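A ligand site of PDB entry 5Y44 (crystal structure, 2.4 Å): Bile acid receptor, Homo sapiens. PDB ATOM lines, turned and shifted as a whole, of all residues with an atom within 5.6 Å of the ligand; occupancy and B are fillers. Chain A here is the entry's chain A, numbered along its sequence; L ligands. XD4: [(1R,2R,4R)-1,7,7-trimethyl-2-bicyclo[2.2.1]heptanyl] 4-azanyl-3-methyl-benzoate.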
ATOM      1  N   PHE A  41      22.279 -21.903  16.090  1.00  0.00           N
ATOM      2  CA  PHE A  41      23.196 -21.673  14.990  1.00  0.00           C
ATOM      3  C   PHE A  41      22.464 -21.537  13.644  1.00  0.00           C
ATOM      4  O   PHE A  41      22.821 -20.675  12.856  1.00  0.00           O
ATOM      5  CB  PHE A  41      24.296 -22.751  14.901  1.00  0.00           C
ATOM      6  CG  PHE A  41      25.219 -22.584  13.704  1.00  0.00           C
ATOM      7  CD1 PHE A  41      26.286 -21.704  13.752  1.00  0.00           C
ATOM      8  CD2 PHE A  41      24.989 -23.284  12.516  1.00  0.00           C
ATOM      9  CE1 PHE A  41      27.118 -21.520  12.640  1.00  0.00           C
ATOM     10  CE2 PHE A  41      25.803 -23.116  11.401  1.00  0.00           C
ATOM     11  CZ  PHE A  41      26.891 -22.248  11.482  1.00  0.00           C
ATOM     12  N   LEU A  44      20.943 -17.979  13.662  1.00  0.00           N
ATOM     13  CA  LEU A  44      21.977 -17.033  13.487  1.00  0.00           C
ATOM     14  C   LEU A  44      22.538 -16.995  12.084  1.00  0.00           C
ATOM     15  O   LEU A  44      22.863 -15.903  11.592  1.00  0.00           O
ATOM     16  CB  LEU A  44      23.086 -17.312  14.491  1.00  0.00           C
ATOM     17  CG  LEU A  44      22.719 -17.223  15.977  1.00  0.00           C
ATOM     18  CD1 LEU A  44      24.004 -17.183  16.800  1.00  0.00           C
ATOM     19  CD2 LEU A  44      21.868 -16.006  16.297  1.00  0.00           C
ATOM     20  N   THR A  45      22.619 -18.158  11.442  1.00  0.00           N
ATOM     21  CA  THR A  45      23.060 -18.232  10.059  1.00  0.00           C
ATOM     22  C   THR A  45      22.098 -17.436   9.222  1.00  0.00           C
ATOM     23  O   THR A  45      22.491 -16.576   8.465  1.00  0.00           O
ATOM     24  CB  THR A  45      23.181 -19.670   9.596  1.00  0.00           C
ATOM     25  OG1 THR A  45      24.254 -20.242  10.319  1.00  0.00           O
ATOM     26  CG2 THR A  45      23.474 -19.763   8.144  1.00  0.00           C
ATOM     27  N   MET A  47      19.952 -15.040  10.193  1.00  0.00           N
ATOM     28  CA  MET A  47      20.082 -13.613  10.517  1.00  0.00           C
ATOM     29  C   MET A  47      21.294 -12.940   9.876  1.00  0.00           C
ATOM     30  O   MET A  47      21.152 -11.873   9.301  1.00  0.00           O
ATOM     31  CB  MET A  47      20.255 -13.383  12.023  1.00  0.00           C
ATOM     32  CG  MET A  47      18.945 -13.429  12.768  1.00  0.00           C
ATOM     33  SD  MET A  47      19.323 -13.005  14.485  1.00  0.00           S
ATOM     34  CE  MET A  47      19.601 -11.242  14.445  1.00  0.00           C
ATOM     35  N   ALA A  48      22.434 -13.598   9.935  1.00  0.00           N
ATOM     36  CA  ALA A  48      23.648 -13.084   9.313  1.00  0.00           C
ATOM     37  C   ALA A  48      23.441 -12.934   7.848  1.00  0.00           C
ATOM     38  O   ALA A  48      23.729 -11.908   7.274  1.00  0.00           O
ATOM     39  CB  ALA A  48      24.888 -13.947   9.630  1.00  0.00           C
ATOM     40  N   HIS A  51      21.315  -9.885   7.324  1.00  0.00           N
ATOM     41  CA  HIS A  51      22.112  -8.673   7.511  1.00  0.00           C
ATOM     42  C   HIS A  51      22.945  -8.339   6.258  1.00  0.00           C
ATOM     43  O   HIS A  51      22.960  -7.223   5.827  1.00  0.00           O
ATOM     44  CB  HIS A  51      23.080  -8.814   8.670  1.00  0.00           C
ATOM     45  CG  HIS A  51      22.456  -8.809  10.029  1.00  0.00           C
ATOM     46  ND1 HIS A  51      21.186  -8.371  10.272  1.00  0.00           N
ATOM     47  CD2 HIS A  51      22.939  -9.212  11.226  1.00  0.00           C
ATOM     48  CE1 HIS A  51      20.906  -8.513  11.561  1.00  0.00           C
ATOM     49  NE2 HIS A  51      21.974  -9.007  12.164  1.00  0.00           N
ATOM     50  N   MET A  85      27.621  -5.165   9.662  1.00  0.00           N
ATOM     51  CA  MET A  85      26.749  -6.101  10.320  1.00  0.00           C
ATOM     52  C   MET A  85      26.708  -5.932  11.878  1.00  0.00           C
ATOM     53  O   MET A  85      25.619  -5.901  12.483  1.00  0.00           O
ATOM     54  CB  MET A  85      27.188  -7.527   9.915  1.00  0.00           C
ATOM     55  CG  MET A  85      26.378  -8.613  10.611  1.00  0.00           C
ATOM     56  SD  MET A  85      26.898 -10.221  10.070  1.00  0.00           S
ATOM     57  CE  MET A  85      28.595 -10.414  10.603  1.00  0.00           C
ATOM     58  N   PHE A  86      27.863  -5.887  12.528  1.00  0.00           N
ATOM     59  CA  PHE A  86      27.866  -5.688  13.990  1.00  0.00           C
ATOM     60  C   PHE A  86      27.180  -4.450  14.434  1.00  0.00           C
ATOM     61  O   PHE A  86      26.542  -4.413  15.485  1.00  0.00           O
ATOM     62  CB  PHE A  86      29.273  -5.742  14.536  1.00  0.00           C
ATOM     63  CG  PHE A  86      29.704  -7.141  14.862  1.00  0.00           C
ATOM     64  CD1 PHE A  86      29.402  -7.688  16.091  1.00  0.00           C
ATOM     65  CD2 PHE A  86      30.346  -7.920  13.946  1.00  0.00           C
ATOM     66  CE1 PHE A  86      29.748  -8.996  16.395  1.00  0.00           C
ATOM     67  CE2 PHE A  86      30.709  -9.236  14.233  1.00  0.00           C
ATOM     68  CZ  PHE A  86      30.424  -9.767  15.465  1.00  0.00           C
ATOM     69  N   SER A  89      23.481  -5.071  14.080  1.00  0.00           N
ATOM     70  CA  SER A  89      22.938  -5.962  15.128  1.00  0.00           C
ATOM     71  C   SER A  89      22.797  -5.207  16.478  1.00  0.00           C
ATOM     72  O   SER A  89      21.812  -5.402  17.184  1.00  0.00           O
ATOM     73  CB  SER A  89      23.754  -7.217  15.269  1.00  0.00           C
ATOM     74  OG  SER A  89      25.024  -6.886  15.713  1.00  0.00           O
ATOM     75  N   ILE A 109      22.370 -16.636  21.039  1.00  0.00           N
ATOM     76  CA  ILE A 109      23.734 -16.271  20.713  1.00  0.00           C
ATOM     77  C   ILE A 109      24.710 -16.964  21.669  1.00  0.00           C
ATOM     78  O   ILE A 109      25.744 -17.441  21.235  1.00  0.00           O
ATOM     79  CB  ILE A 109      23.908 -14.741  20.793  1.00  0.00           C
ATOM     80  CG1 ILE A 109      23.142 -14.070  19.670  1.00  0.00           C
ATOM     81  CG2 ILE A 109      25.379 -14.361  20.665  1.00  0.00           C
ATOM     82  CD1 ILE A 109      23.127 -12.551  19.744  1.00  0.00           C
ATOM     83  N   ILE A 114      29.756 -20.537  19.999  1.00  0.00           N
ATOM     84  CA  ILE A 114      30.659 -19.399  20.060  1.00  0.00           C
ATOM     85  C   ILE A 114      31.278 -19.357  21.482  1.00  0.00           C
ATOM     86  O   ILE A 114      30.548 -19.295  22.509  1.00  0.00           O
ATOM     87  CB  ILE A 114      29.967 -18.042  19.792  1.00  0.00           C
ATOM     88  CG1 ILE A 114      29.110 -18.080  18.543  1.00  0.00           C
ATOM     89  CG2 ILE A 114      31.000 -16.936  19.598  1.00  0.00           C
ATOM     90  CD1 ILE A 114      28.215 -16.869  18.354  1.00  0.00           C
ATOM     91  N   MET A 122      31.288  -8.806  22.291  1.00  0.00           N
ATOM     92  CA  MET A 122      30.171  -8.521  21.467  1.00  0.00           C
ATOM     93  C   MET A 122      29.215  -7.771  22.327  1.00  0.00           C
ATOM     94  O   MET A 122      28.858  -6.669  22.005  1.00  0.00           O
ATOM     95  CB  MET A 122      29.619  -9.815  20.897  1.00  0.00           C
ATOM     96  CG  MET A 122      28.357  -9.778  20.086  1.00  0.00           C
ATOM     97  SD  MET A 122      27.807 -11.469  19.531  1.00  0.00           S
ATOM     98  CE  MET A 122      29.396 -12.153  19.084  1.00  0.00           C
ATOM     99  N   TYR A 126      27.639  -3.838  22.404  1.00  0.00           N
ATOM    100  CA  TYR A 126      26.221  -3.474  22.410  1.00  0.00           C
ATOM    101  C   TYR A 126      25.862  -2.460  23.508  1.00  0.00           C
ATOM    102  O   TYR A 126      25.007  -1.597  23.303  1.00  0.00           O
ATOM    103  CB  TYR A 126      25.329  -4.745  22.530  1.00  0.00           C
ATOM    104  CG  TYR A 126      25.316  -5.709  21.334  1.00  0.00           C
ATOM    105  CD1 TYR A 126      25.754  -5.321  20.060  1.00  0.00           C
ATOM    106  CD2 TYR A 126      24.816  -7.011  21.467  1.00  0.00           C
ATOM    107  CE1 TYR A 126      25.741  -6.196  19.009  1.00  0.00           C
ATOM    108  CE2 TYR A 126      24.778  -7.886  20.398  1.00  0.00           C
ATOM    109  CZ  TYR A 126      25.237  -7.462  19.168  1.00  0.00           C
ATOM    110  OH  TYR A 126      25.220  -8.251  18.068  1.00  0.00           O
ATOM    111  N   HIS A 204      35.721 -11.942  14.311  1.00  0.00           N
ATOM    112  CA  HIS A 204      34.794 -12.612  13.458  1.00  0.00           C
ATOM    113  C   HIS A 204      35.525 -13.686  12.665  1.00  0.00           C
ATOM    114  O   HIS A 204      34.992 -14.782  12.465  1.00  0.00           O
ATOM    115  CB  HIS A 204      34.052 -11.624  12.530  1.00  0.00           C
ATOM    116  CG  HIS A 204      32.937 -12.241  11.745  1.00  0.00           C
ATOM    117  ND1 HIS A 204      33.132 -12.818  10.503  1.00  0.00           N
ATOM    118  CD2 HIS A 204      31.634 -12.432  12.063  1.00  0.00           C
ATOM    119  CE1 HIS A 204      31.984 -13.304  10.065  1.00  0.00           C
ATOM    120  NE2 HIS A 204      31.051 -13.069  10.982  1.00  0.00           N
ATOM    121  N   MET A 207      35.813 -16.620  15.024  1.00  0.00           N
ATOM    122  CA  MET A 207      34.564 -17.348  15.108  1.00  0.00           C
ATOM    123  C   MET A 207      34.306 -18.240  13.895  1.00  0.00           C
ATOM    124  O   MET A 207      33.838 -19.391  14.047  1.00  0.00           O
ATOM    125  CB  MET A 207      33.398 -16.399  15.188  1.00  0.00           C
ATOM    126  CG  MET A 207      33.213 -15.744  16.517  1.00  0.00           C
ATOM    127  SD  MET A 207      31.671 -14.830  16.321  1.00  0.00           S
ATOM    128  CE  MET A 207      32.373 -13.206  16.384  1.00  0.00           C
ATOM    129  N   LEU A 208      34.523 -17.695  12.686  1.00  0.00           N
ATOM    130  CA  LEU A 208      34.364 -18.509  11.488  1.00  0.00           C
ATOM    131  C   LEU A 208      35.311 -19.710  11.453  1.00  0.00           C
ATOM    132  O   LEU A 208      34.918 -20.771  11.027  1.00  0.00           O
ATOM    133  CB  LEU A 208      34.551 -17.724  10.201  1.00  0.00           C
ATOM    134  CG  LEU A 208      33.476 -16.708   9.918  1.00  0.00           C
ATOM    135  CD1 LEU A 208      33.504 -16.379   8.432  1.00  0.00           C
ATOM    136  CD2 LEU A 208      32.082 -17.130  10.360  1.00  0.00           C
ATOM    137  N   TRP A 211      33.839 -22.372  13.899  1.00  0.00           N
ATOM    138  CA  TRP A 211      32.651 -22.956  13.302  1.00  0.00           C
ATOM    139  C   TRP A 211      32.975 -23.965  12.252  1.00  0.00           C
ATOM    140  O   TRP A 211      32.292 -24.991  12.191  1.00  0.00           O
ATOM    141  CB  TRP A 211      31.670 -21.947  12.740  1.00  0.00           C
ATOM    142  CG  TRP A 211      30.747 -21.403  13.754  1.00  0.00           C
ATOM    143  CD1 TRP A 211      30.230 -22.065  14.867  1.00  0.00           C
ATOM    144  CD2 TRP A 211      30.182 -20.111  13.765  1.00  0.00           C
ATOM    145  NE1 TRP A 211      29.396 -21.233  15.558  1.00  0.00           N
ATOM    146  CE2 TRP A 211      29.331 -20.033  14.896  1.00  0.00           C
ATOM    147  CE3 TRP A 211      30.293 -19.007  12.911  1.00  0.00           C
ATOM    148  CZ2 TRP A 211      28.620 -18.847  15.219  1.00  0.00           C
ATOM    149  CZ3 TRP A 211      29.551 -17.842  13.226  1.00  0.00           C
ATOM    150  CH2 TRP A 211      28.739 -17.777  14.366  1.00  0.00           C
ATOM    151  N   LYS A 216      28.092 -25.656   7.943  1.00  0.00           N
ATOM    152  CA  LYS A 216      27.688 -25.305   6.594  1.00  0.00           C
ATOM    153  C   LYS A 216      27.131 -23.858   6.586  1.00  0.00           C
ATOM    154  O   LYS A 216      26.429 -23.423   7.559  1.00  0.00           O
ATOM    155  CB  LYS A 216      26.662 -26.325   6.027  1.00  0.00           C
ATOM    156  CG  LYS A 216      25.907 -27.214   7.037  1.00  0.00           C
ATOM    157  CD  LYS A 216      24.831 -26.488   7.881  1.00  0.00           C
ATOM    158  CE  LYS A 216      24.504 -27.203   9.206  1.00  0.00           C
ATOM    159  NZ  LYS A 216      25.080 -26.539  10.408  1.00  0.00           N
ATOM    160  N   PHE A 217      27.478 -23.122   5.522  1.00  0.00           N
ATOM    161  CA  PHE A 217      27.082 -21.714   5.362  1.00  0.00           C
ATOM    162  C   PHE A 217      26.293 -21.451   4.102  1.00  0.00           C
ATOM    163  O   PHE A 217      26.500 -22.108   3.043  1.00  0.00           O
ATOM    164  CB  PHE A 217      28.306 -20.789   5.296  1.00  0.00           C
ATOM    165  CG  PHE A 217      29.233 -20.874   6.465  1.00  0.00           C
ATOM    166  CD1 PHE A 217      28.844 -21.370   7.704  1.00  0.00           C
ATOM    167  CD2 PHE A 217      30.530 -20.410   6.329  1.00  0.00           C
ATOM    168  CE1 PHE A 217      29.717 -21.395   8.768  1.00  0.00           C
ATOM    169  CE2 PHE A 217      31.423 -20.436   7.383  1.00  0.00           C
ATOM    170  CZ  PHE A 217      31.019 -20.937   8.603  1.00  0.00           C
ATOM    171  N   LEU A 221      27.093 -15.949   2.471  1.00  0.00           N
ATOM    172  CA  LEU A 221      28.078 -15.789   3.469  1.00  0.00           C
ATOM    173  C   LEU A 221      29.381 -16.399   3.011  1.00  0.00           C
ATOM    174  O   LEU A 221      30.450 -15.933   3.405  1.00  0.00           O
ATOM    175  CB  LEU A 221      27.626 -16.476   4.753  1.00  0.00           C
ATOM    176  CG  LEU A 221      26.332 -15.897   5.291  1.00  0.00           C
ATOM    177  CD1 LEU A 221      25.913 -16.564   6.597  1.00  0.00           C
ATOM    178  CD2 LEU A 221      26.466 -14.396   5.494  1.00  0.00           C
ATOM    179  N   TRP A 225      32.575 -13.662   2.681  1.00  0.00           N
ATOM    180  CA  TRP A 225      33.808 -13.885   3.446  1.00  0.00           C
ATOM    181  C   TRP A 225      34.827 -14.859   2.874  1.00  0.00           C
ATOM    182  O   TRP A 225      35.714 -15.191   3.579  1.00  0.00           O
ATOM    183  CB  TRP A 225      33.447 -14.266   4.880  1.00  0.00           C
ATOM    184  CG  TRP A 225      32.827 -13.153   5.560  1.00  0.00           C
ATOM    185  CD1 TRP A 225      33.284 -11.872   5.593  1.00  0.00           C
ATOM    186  CD2 TRP A 225      31.609 -13.169   6.332  1.00  0.00           C
ATOM    187  NE1 TRP A 225      32.436 -11.108   6.306  1.00  0.00           N
ATOM    188  CE2 TRP A 225      31.397 -11.866   6.776  1.00  0.00           C
ATOM    189  CE3 TRP A 225      30.678 -14.174   6.660  1.00  0.00           C
ATOM    190  CZ2 TRP A 225      30.280 -11.498   7.517  1.00  0.00           C
ATOM    191  CZ3 TRP A 225      29.576 -13.817   7.471  1.00  0.00           C
ATOM    192  CH2 TRP A 225      29.384 -12.476   7.859  1.00  0.00           C
HETATM  193  O1  XD4 L   1      28.855 -13.786  12.267  1.00  0.00           O
HETATM  194  C3  XD4 L   1      27.725 -14.153  12.025  1.00  0.00           C
HETATM  195  C4  XD4 L   1      27.470 -15.508  11.414  1.00  0.00           C
HETATM  196  C10 XD4 L   1      26.470 -16.320  11.939  1.00  0.00           C
HETATM  197  C9  XD4 L   1      26.210 -17.573  11.392  1.00  0.00           C
HETATM  198  C8  XD4 L   1      26.963 -18.041  10.328  1.00  0.00           C
HETATM  199  N   XD4 L   1      26.720 -19.259   9.797  1.00  0.00           N
HETATM  200  C6  XD4 L   1      28.038 -17.171   9.772  1.00  0.00           C
HETATM  201  C7  XD4 L   1      28.875 -17.646   8.616  1.00  0.00           C
HETATM  202  C5  XD4 L   1      28.253 -15.928  10.341  1.00  0.00           C
HETATM  203  O   XD4 L   1      26.601 -13.275  12.327  1.00  0.00           O
HETATM  204  C2  XD4 L   1      26.072 -13.523  13.627  1.00  0.00           C
HETATM  205  C11 XD4 L   1      24.601 -13.146  13.683  1.00  0.00           C
HETATM  206  C12 XD4 L   1      24.557 -12.030  14.704  1.00  0.00           C
HETATM  207  C13 XD4 L   1      25.871 -11.341  14.476  1.00  0.00           C
HETATM  208  C15 XD4 L   1      26.167 -10.319  15.566  1.00  0.00           C
HETATM  209  C14 XD4 L   1      25.985 -10.726  13.084  1.00  0.00           C
HETATM  210  C16 XD4 L   1      24.784 -12.702  16.054  1.00  0.00           C
HETATM  211  C17 XD4 L   1      26.271 -13.075  16.016  1.00  0.00           C
HETATM  212  C1  XD4 L   1      26.706 -12.585  14.641  1.00  0.00           C
HETATM  213  C   XD4 L   1      28.199 -12.378  14.487  1.00  0.00           C
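Residues that only touch the ligand: Met 85 (3.2 Å), Ala 48 (3.3 Å), Tyr 126 (3.4 Å), Phe 41 (3.4 Å), Phe 86 (3.6 Å), Trp 211 (3.6 Å), Ser 89 (3.6 Å), Leu 44 (3.6 Å), Phe 217 (3.7 Å), Leu 208 (3.7 Å), Leu 221 (3.7 Å), Trp 225 (3.8 Å) and His 51 (3.9 Å). Of the 21 residues printed, 15 come within 4 Å of the ligand. Along chain A the residues within 4 Å of the ligand span positions 41 to 225. The nearest printed residue that does not touch the ligand is Ile 109 (4.05 Å).
A ring nitrogen (NE2) of His 204 sits at hydrogen-bond distance from an oxygen (O1) of the ligand, at 2.6 Å. OG1 of Thr 45 is in hydrogen-bond range of N of the ligand (2.7 Å).
The side-chain hydroxyl (OG1) of Thr 45 is in hydrogen-bond range of the backbone carbonyl oxygen (O) of Phe 41 (2.9 Å). The side-chain hydroxyl of Ser 89 is in hydrogen-bond range of the backbone carbonyl oxygen of Met 85 (3.4 Å). The side-chain hydroxyl of Ser 89 lies within hydrogen-bond range of the side-chain hydroxyl of Tyr 126 (2.7 Å). OG of Ser 89 is in hydrogen-bond range of O of Phe 86, at 2.9 Å.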
